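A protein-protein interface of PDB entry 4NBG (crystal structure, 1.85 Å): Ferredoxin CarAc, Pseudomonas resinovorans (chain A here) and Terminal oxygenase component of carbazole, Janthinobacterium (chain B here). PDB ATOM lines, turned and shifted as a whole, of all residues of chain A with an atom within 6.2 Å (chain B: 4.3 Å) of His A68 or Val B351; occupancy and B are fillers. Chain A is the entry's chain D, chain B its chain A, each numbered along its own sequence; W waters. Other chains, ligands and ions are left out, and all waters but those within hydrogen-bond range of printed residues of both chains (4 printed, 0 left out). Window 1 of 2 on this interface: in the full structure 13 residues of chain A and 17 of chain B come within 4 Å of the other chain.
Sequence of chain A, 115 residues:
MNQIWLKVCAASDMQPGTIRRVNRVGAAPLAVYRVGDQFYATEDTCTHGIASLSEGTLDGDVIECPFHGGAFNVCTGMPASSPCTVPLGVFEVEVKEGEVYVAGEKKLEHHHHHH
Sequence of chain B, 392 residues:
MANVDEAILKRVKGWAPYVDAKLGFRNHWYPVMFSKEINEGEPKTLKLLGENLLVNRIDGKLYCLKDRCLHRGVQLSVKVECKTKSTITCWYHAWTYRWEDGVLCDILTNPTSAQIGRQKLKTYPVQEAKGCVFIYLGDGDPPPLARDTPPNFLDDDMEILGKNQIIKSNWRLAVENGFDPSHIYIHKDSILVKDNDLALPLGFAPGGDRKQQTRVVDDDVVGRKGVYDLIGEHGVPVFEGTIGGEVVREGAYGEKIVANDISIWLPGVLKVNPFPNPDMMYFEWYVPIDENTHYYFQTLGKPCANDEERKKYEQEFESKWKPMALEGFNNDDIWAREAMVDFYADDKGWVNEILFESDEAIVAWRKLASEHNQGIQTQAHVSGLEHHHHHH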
ATOM      1  N   HIS A  48      35.114  15.246 -24.510  1.00  0.00           N
ATOM      2  CA  HIS A  48      33.713  14.969 -24.204  1.00  0.00           C
ATOM      3  C   HIS A  48      32.764  15.436 -25.314  1.00  0.00           C
ATOM      4  O   HIS A  48      31.566  15.149 -25.279  1.00  0.00           O
ATOM      5  CB  HIS A  48      33.333  15.637 -22.874  1.00  0.00           C
ATOM      6  CG  HIS A  48      31.894  15.462 -22.492  1.00  0.00           C
ATOM      7  ND1 HIS A  48      30.966  16.476 -22.595  1.00  0.00           N
ATOM      8  CD2 HIS A  48      31.225  14.389 -22.005  1.00  0.00           C
ATOM      9  CE1 HIS A  48      29.788  16.038 -22.185  1.00  0.00           C
ATOM     10  NE2 HIS A  48      29.918  14.774 -21.821  1.00  0.00           N
ATOM     11  N   GLY A  49      33.296  16.151 -26.298  1.00  0.00           N
ATOM     12  CA  GLY A  49      32.449  16.632 -27.374  1.00  0.00           C
ATOM     13  C   GLY A  49      33.192  17.256 -28.536  1.00  0.00           C
ATOM     14  O   GLY A  49      34.096  16.648 -29.104  1.00  0.00           O
ATOM     15  N   CYS A  65      36.205  23.304 -19.701  1.00  0.00           N
ATOM     16  CA  CYS A  65      35.541  23.354 -21.000  1.00  0.00           C
ATOM     17  C   CYS A  65      34.334  24.290 -20.955  1.00  0.00           C
ATOM     18  O   CYS A  65      33.535  24.233 -20.026  1.00  0.00           O
ATOM     19  CB  CYS A  65      35.088  21.952 -21.405  1.00  0.00           C
ATOM     20  SG  CYS A  65      34.231  21.919 -22.979  1.00  0.00           S
ATOM     21  N   PRO A  66      34.179  25.152 -21.975  1.00  0.00           N
ATOM     22  CA  PRO A  66      33.065  26.104 -22.039  1.00  0.00           C
ATOM     23  C   PRO A  66      31.693  25.501 -22.335  1.00  0.00           C
ATOM     24  O   PRO A  66      30.666  26.130 -22.080  1.00  0.00           O
ATOM     25  CB  PRO A  66      33.518  27.078 -23.121  1.00  0.00           C
ATOM     26  CG  PRO A  66      34.257  26.190 -24.061  1.00  0.00           C
ATOM     27  CD  PRO A  66      35.081  25.331 -23.127  1.00  0.00           C
ATOM     28  N   PHE A  67      31.674  24.282 -22.865  1.00  0.00           N
ATOM     29  CA  PHE A  67      30.417  23.623 -23.201  1.00  0.00           C
ATOM     30  C   PHE A  67      29.636  23.112 -22.000  1.00  0.00           C
ATOM     31  O   PHE A  67      28.505  23.543 -21.760  1.00  0.00           O
ATOM     32  CB  PHE A  67      30.673  22.451 -24.157  1.00  0.00           C
ATOM     33  CG  PHE A  67      30.634  22.826 -25.615  1.00  0.00           C
ATOM     34  CD1 PHE A  67      30.979  24.105 -26.039  1.00  0.00           C
ATOM     35  CD2 PHE A  67      30.294  21.875 -26.573  1.00  0.00           C
ATOM     36  CE1 PHE A  67      30.990  24.431 -27.400  1.00  0.00           C
ATOM     37  CE2 PHE A  67      30.302  22.189 -27.932  1.00  0.00           C
ATOM     38  CZ  PHE A  67      30.652  23.468 -28.345  1.00  0.00           C
ATOM     39  N   HIS A  68      30.235  22.196 -21.242  1.00  0.00           N
ATOM     40  CA  HIS A  68      29.542  21.614 -20.100  1.00  0.00           C
ATOM     41  C   HIS A  68      30.242  21.732 -18.751  1.00  0.00           C
ATOM     42  O   HIS A  68      29.757  21.207 -17.753  1.00  0.00           O
ATOM     43  CB  HIS A  68      29.241  20.141 -20.386  1.00  0.00           C
ATOM     44  CG  HIS A  68      28.648  19.901 -21.738  1.00  0.00           C
ATOM     45  ND1 HIS A  68      29.344  19.288 -22.758  1.00  0.00           N
ATOM     46  CD2 HIS A  68      27.429  20.207 -22.245  1.00  0.00           C
ATOM     47  CE1 HIS A  68      28.579  19.226 -23.833  1.00  0.00           C
ATOM     48  NE2 HIS A  68      27.411  19.777 -23.549  1.00  0.00           N
ATOM     49  N   GLY A  69      31.379  22.416 -18.709  1.00  0.00           N
ATOM     50  CA  GLY A  69      32.069  22.571 -17.439  1.00  0.00           C
ATOM     51  C   GLY A  69      32.991  21.427 -17.055  1.00  0.00           C
ATOM     52  O   GLY A  69      33.459  21.358 -15.914  1.00  0.00           O
ATOM     53  N   GLY A  70      33.234  20.511 -17.985  1.00  0.00           N
ATOM     54  CA  GLY A  70      34.150  19.421 -17.702  1.00  0.00           C
ATOM     55  C   GLY A  70      35.525  20.063 -17.631  1.00  0.00           C
ATOM     56  O   GLY A  70      35.688  21.205 -18.066  1.00  0.00           O
ATOM     57  N   SER A  82      33.811  16.286 -13.951  1.00  0.00           N
ATOM     58  CA  SER A  82      32.830  15.601 -14.785  1.00  0.00           C
ATOM     59  C   SER A  82      32.282  16.699 -15.697  1.00  0.00           C
ATOM     60  O   SER A  82      32.407  17.886 -15.384  1.00  0.00           O
ATOM     61  CB  SER A  82      31.709  15.024 -13.920  1.00  0.00           C
ATOM     62  OG  SER A  82      31.119  16.036 -13.123  1.00  0.00           O
ATOM     63  N   PRO A  83      31.659  16.327 -16.826  1.00  0.00           N
ATOM     64  CA  PRO A  83      31.406  14.971 -17.326  1.00  0.00           C
ATOM     65  C   PRO A  83      32.570  14.295 -18.062  1.00  0.00           C
ATOM     66  O   PRO A  83      32.436  13.162 -18.523  1.00  0.00           O
ATOM     67  CB  PRO A  83      30.202  15.175 -18.240  1.00  0.00           C
ATOM     68  CG  PRO A  83      30.516  16.509 -18.868  1.00  0.00           C
ATOM     69  CD  PRO A  83      30.988  17.334 -17.673  1.00  0.00           C
ATOM     70  N   ILE B   8      23.640  24.039 -12.946  1.00  0.00           N
ATOM     71  CA  ILE B   8      23.661  23.558 -14.319  1.00  0.00           C
ATOM     72  C   ILE B   8      23.897  24.729 -15.266  1.00  0.00           C
ATOM     73  O   ILE B   8      24.720  24.644 -16.183  1.00  0.00           O
ATOM     74  CB  ILE B   8      22.333  22.858 -14.683  1.00  0.00           C
ATOM     75  CG1 ILE B   8      22.175  21.586 -13.843  1.00  0.00           C
ATOM     76  CG2 ILE B   8      22.303  22.533 -16.171  1.00  0.00           C
ATOM     77  CD1 ILE B   8      20.860  20.863 -14.056  1.00  0.00           C
ATOM     78  N   ARG B  11      27.409  25.747 -15.654  1.00  0.00           N
ATOM     79  CA  ARG B  11      28.220  24.847 -16.471  1.00  0.00           C
ATOM     80  C   ARG B  11      28.109  25.076 -17.979  1.00  0.00           C
ATOM     81  O   ARG B  11      29.097  24.946 -18.700  1.00  0.00           O
ATOM     82  CB  ARG B  11      27.863  23.392 -16.160  1.00  0.00           C
ATOM     83  CG  ARG B  11      28.605  22.800 -14.969  1.00  0.00           C
ATOM     84  CD  ARG B  11      28.054  21.428 -14.614  1.00  0.00           C
ATOM     85  NE  ARG B  11      28.913  20.712 -13.675  1.00  0.00           N
ATOM     86  CZ  ARG B  11      30.023  20.060 -14.016  1.00  0.00           C
ATOM     87  NH1 ARG B  11      30.420  20.021 -15.284  1.00  0.00           N
ATOM     88  NH2 ARG B  11      30.738  19.445 -13.085  1.00  0.00           N
ATOM     89  N   LYS B 348      19.817  17.391 -16.781  1.00  0.00           N
ATOM     90  CA  LYS B 348      21.188  16.887 -16.773  1.00  0.00           C
ATOM     91  C   LYS B 348      21.722  16.537 -18.163  1.00  0.00           C
ATOM     92  O   LYS B 348      22.931  16.534 -18.380  1.00  0.00           O
ATOM     93  CB  LYS B 348      21.308  15.671 -15.841  1.00  0.00           C
ATOM     94  CG  LYS B 348      21.037  15.976 -14.362  1.00  0.00           C
ATOM     95  CD  LYS B 348      21.969  17.064 -13.831  1.00  0.00           C
ATOM     96  CE  LYS B 348      21.651  17.433 -12.376  1.00  0.00           C
ATOM     97  NZ  LYS B 348      21.911  16.324 -11.413  1.00  0.00           N
ATOM     98  N   GLY B 349      20.830  16.250 -19.106  1.00  0.00           N
ATOM     99  CA  GLY B 349      21.282  15.924 -20.449  1.00  0.00           C
ATOM    100  C   GLY B 349      22.045  17.071 -21.094  1.00  0.00           C
ATOM    101  O   GLY B 349      22.885  16.857 -21.970  1.00  0.00           O
ATOM    102  N   TRP B 350      21.754  18.295 -20.663  1.00  0.00           N
ATOM    103  CA  TRP B 350      22.420  19.477 -21.206  1.00  0.00           C
ATOM    104  C   TRP B 350      23.881  19.518 -20.781  1.00  0.00           C
ATOM    105  O   TRP B 350      24.662  20.324 -21.290  1.00  0.00           O
ATOM    106  CB  TRP B 350      21.725  20.757 -20.739  1.00  0.00           C
ATOM    107  CG  TRP B 350      20.287  20.852 -21.150  1.00  0.00           C
ATOM    108  CD1 TRP B 350      19.195  20.781 -20.329  1.00  0.00           C
ATOM    109  CD2 TRP B 350      19.780  21.043 -22.476  1.00  0.00           C
ATOM    110  NE1 TRP B 350      18.042  20.921 -21.062  1.00  0.00           N
ATOM    111  CE2 TRP B 350      18.370  21.083 -22.384  1.00  0.00           C
ATOM    112  CE3 TRP B 350      20.382  21.186 -23.738  1.00  0.00           C
ATOM    113  CZ2 TRP B 350      17.548  21.260 -23.503  1.00  0.00           C
ATOM    114  CZ3 TRP B 350      19.562  21.363 -24.855  1.00  0.00           C
ATOM    115  CH2 TRP B 350      18.159  21.399 -24.727  1.00  0.00           C
ATOM    116  N   VAL B 351      24.245  18.649 -19.845  1.00  0.00           N
ATOM    117  CA  VAL B 351      25.620  18.578 -19.373  1.00  0.00           C
ATOM    118  C   VAL B 351      26.289  17.279 -19.826  1.00  0.00           C
ATOM    119  O   VAL B 351      27.443  17.283 -20.258  1.00  0.00           O
ATOM    120  CB  VAL B 351      25.690  18.642 -17.828  1.00  0.00           C
ATOM    121  CG1 VAL B 351      27.120  18.385 -17.358  1.00  0.00           C
ATOM    122  CG2 VAL B 351      25.213  20.005 -17.337  1.00  0.00           C
ATOM    123  N   ASN B 352      25.545  16.178 -19.752  1.00  0.00           N
ATOM    124  CA  ASN B 352      26.081  14.858 -20.084  1.00  0.00           C
ATOM    125  C   ASN B 352      26.088  14.382 -21.534  1.00  0.00           C
ATOM    126  O   ASN B 352      26.709  13.366 -21.843  1.00  0.00           O
ATOM    127  CB  ASN B 352      25.395  13.815 -19.203  1.00  0.00           C
ATOM    128  CG  ASN B 352      25.682  14.036 -17.735  1.00  0.00           C
ATOM    129  OD1 ASN B 352      26.838  14.144 -17.341  1.00  0.00           O
ATOM    130  ND2 ASN B 352      24.636  14.104 -16.920  1.00  0.00           N
ATOM    131  N   GLU B 353      25.412  15.106 -22.419  1.00  0.00           N
ATOM    132  CA  GLU B 353      25.375  14.747 -23.836  1.00  0.00           C
ATOM    133  C   GLU B 353      26.801  14.681 -24.394  1.00  0.00           C
ATOM    134  O   GLU B 353      27.658  15.468 -24.000  1.00  0.00           O
ATOM    135  CB  GLU B 353      24.588  15.820 -24.608  1.00  0.00           C
ATOM    136  CG  GLU B 353      25.172  17.222 -24.398  1.00  0.00           C
ATOM    137  CD  GLU B 353      24.372  18.340 -25.044  1.00  0.00           C
ATOM    138  OE1 GLU B 353      23.219  18.102 -25.459  1.00  0.00           O
ATOM    139  OE2 GLU B 353      24.903  19.473 -25.121  1.00  0.00           O
HETATM  140  O   HOH W   1      28.971  12.198 -20.359  1.00  0.00           O
HETATM  141  O   HOH W   2      29.429  16.809 -25.622  1.00  0.00           O
HETATM  142  O   HOH W   3      29.021  17.024 -14.308  1.00  0.00           O
HETATM  143  O   HOH W   4      31.772  25.612 -18.278  1.00  0.00           O
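O of Gly A70 lies within hydrogen-bond range of N of Cys A65, at 2.7 Å.
O of Lys B348 lies within hydrogen-bond range of ND2 of Asn B352.
SG of Cys A65 sits close to N of Phe A67 (3.5 Å).
The guanidinium group (NH1) of Arg B11 is in hydrogen-bond range of the backbone carbonyl oxygen (O) of Gly A69.
The side-chain carboxylate (OE2) of Glu B353 sits at hydrogen-bond distance from a ring nitrogen (NE2) of His A68.
O of Phe A67 lies close to O of Arg B11 (3.4 Å).
The backbone carbonyl oxygen (O) of Glu B353 sits close to a ring nitrogen (NE2) of His A48.
The backbone carbonyl oxygen of His A68 is in hydrogen-bond range of the guanidinium group of Arg B11, at 2.8 Å.
The backbone carbonyl oxygen (O) of Ser A82 is in hydrogen-bond range of the guanidinium group (NH1) of Arg B11 (2.9 Å).
Printed residues of chain A within 4 Å of Arg B11: Pro A66, Phe A67, His A68, Gly A69, Gly A70, Ser A82 and Pro A83.
Of the printed residues of chain A, Trp B350 touches His A68.
Of the printed residues of chain A, Asn B352 touches His A48 (3.5 Å) and Pro A83 (3.6 Å).
The nearest printed residue of chain B that does not touch His A68 is Asn B352 (5.1 Å).
Hydrophobic or aromatic side chains of chain A that line the printed part of chain B: His A48, His A68 and Pro A83.
Hydrophobic or aromatic side chains of chain B that line the printed part of chain A: Val B351.
Among the printed residues, no Asp or Glu carboxylate lies within 4 Å of a Lys or Arg side-chain nitrogen of the other chain.
Water W3 bridges OG of Ser A82 (2.6 Å) and NH2 of Arg B11 (3.2 Å).
Water W2 bridges the backbone carbonyl oxygen (O) of His A48 (2.7 Å) and the backbone carbonyl oxygen (O) of Glu B353 (2.8 Å).
Water W4 lies within hydrogen-bond range of the backbone carbonyl oxygen (O) of Arg B11 (2.8 Å), the backbone carbonyl oxygen (O) of Cys A65 (2.8 Å) and the backbone NH (N) of Gly A69 (3.2 Å).
Water W1 bridges the backbone carbonyl oxygen (O) of Asn B352 (2.9 Å) and a ring nitrogen (NE2) of His A48 (3.1 Å).
Among the printed residues, merely in contact across the chains: His A68 with Trp B350 (2.9 Å), His A68 with Val B351 (3.2 Å), His A48 with Val B351 (3.3 Å), Pro A83 with Val B351 (3.5 Å), His A48 with Asn B352 (3.5 Å), Pro A83 with Asn B352 (3.6 Å), Pro A83 with Arg B11 (3.6 Å), Pro A66 with Arg B11 (3.9 Å) and Gly A70 with Arg B11 (3.9 Å).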
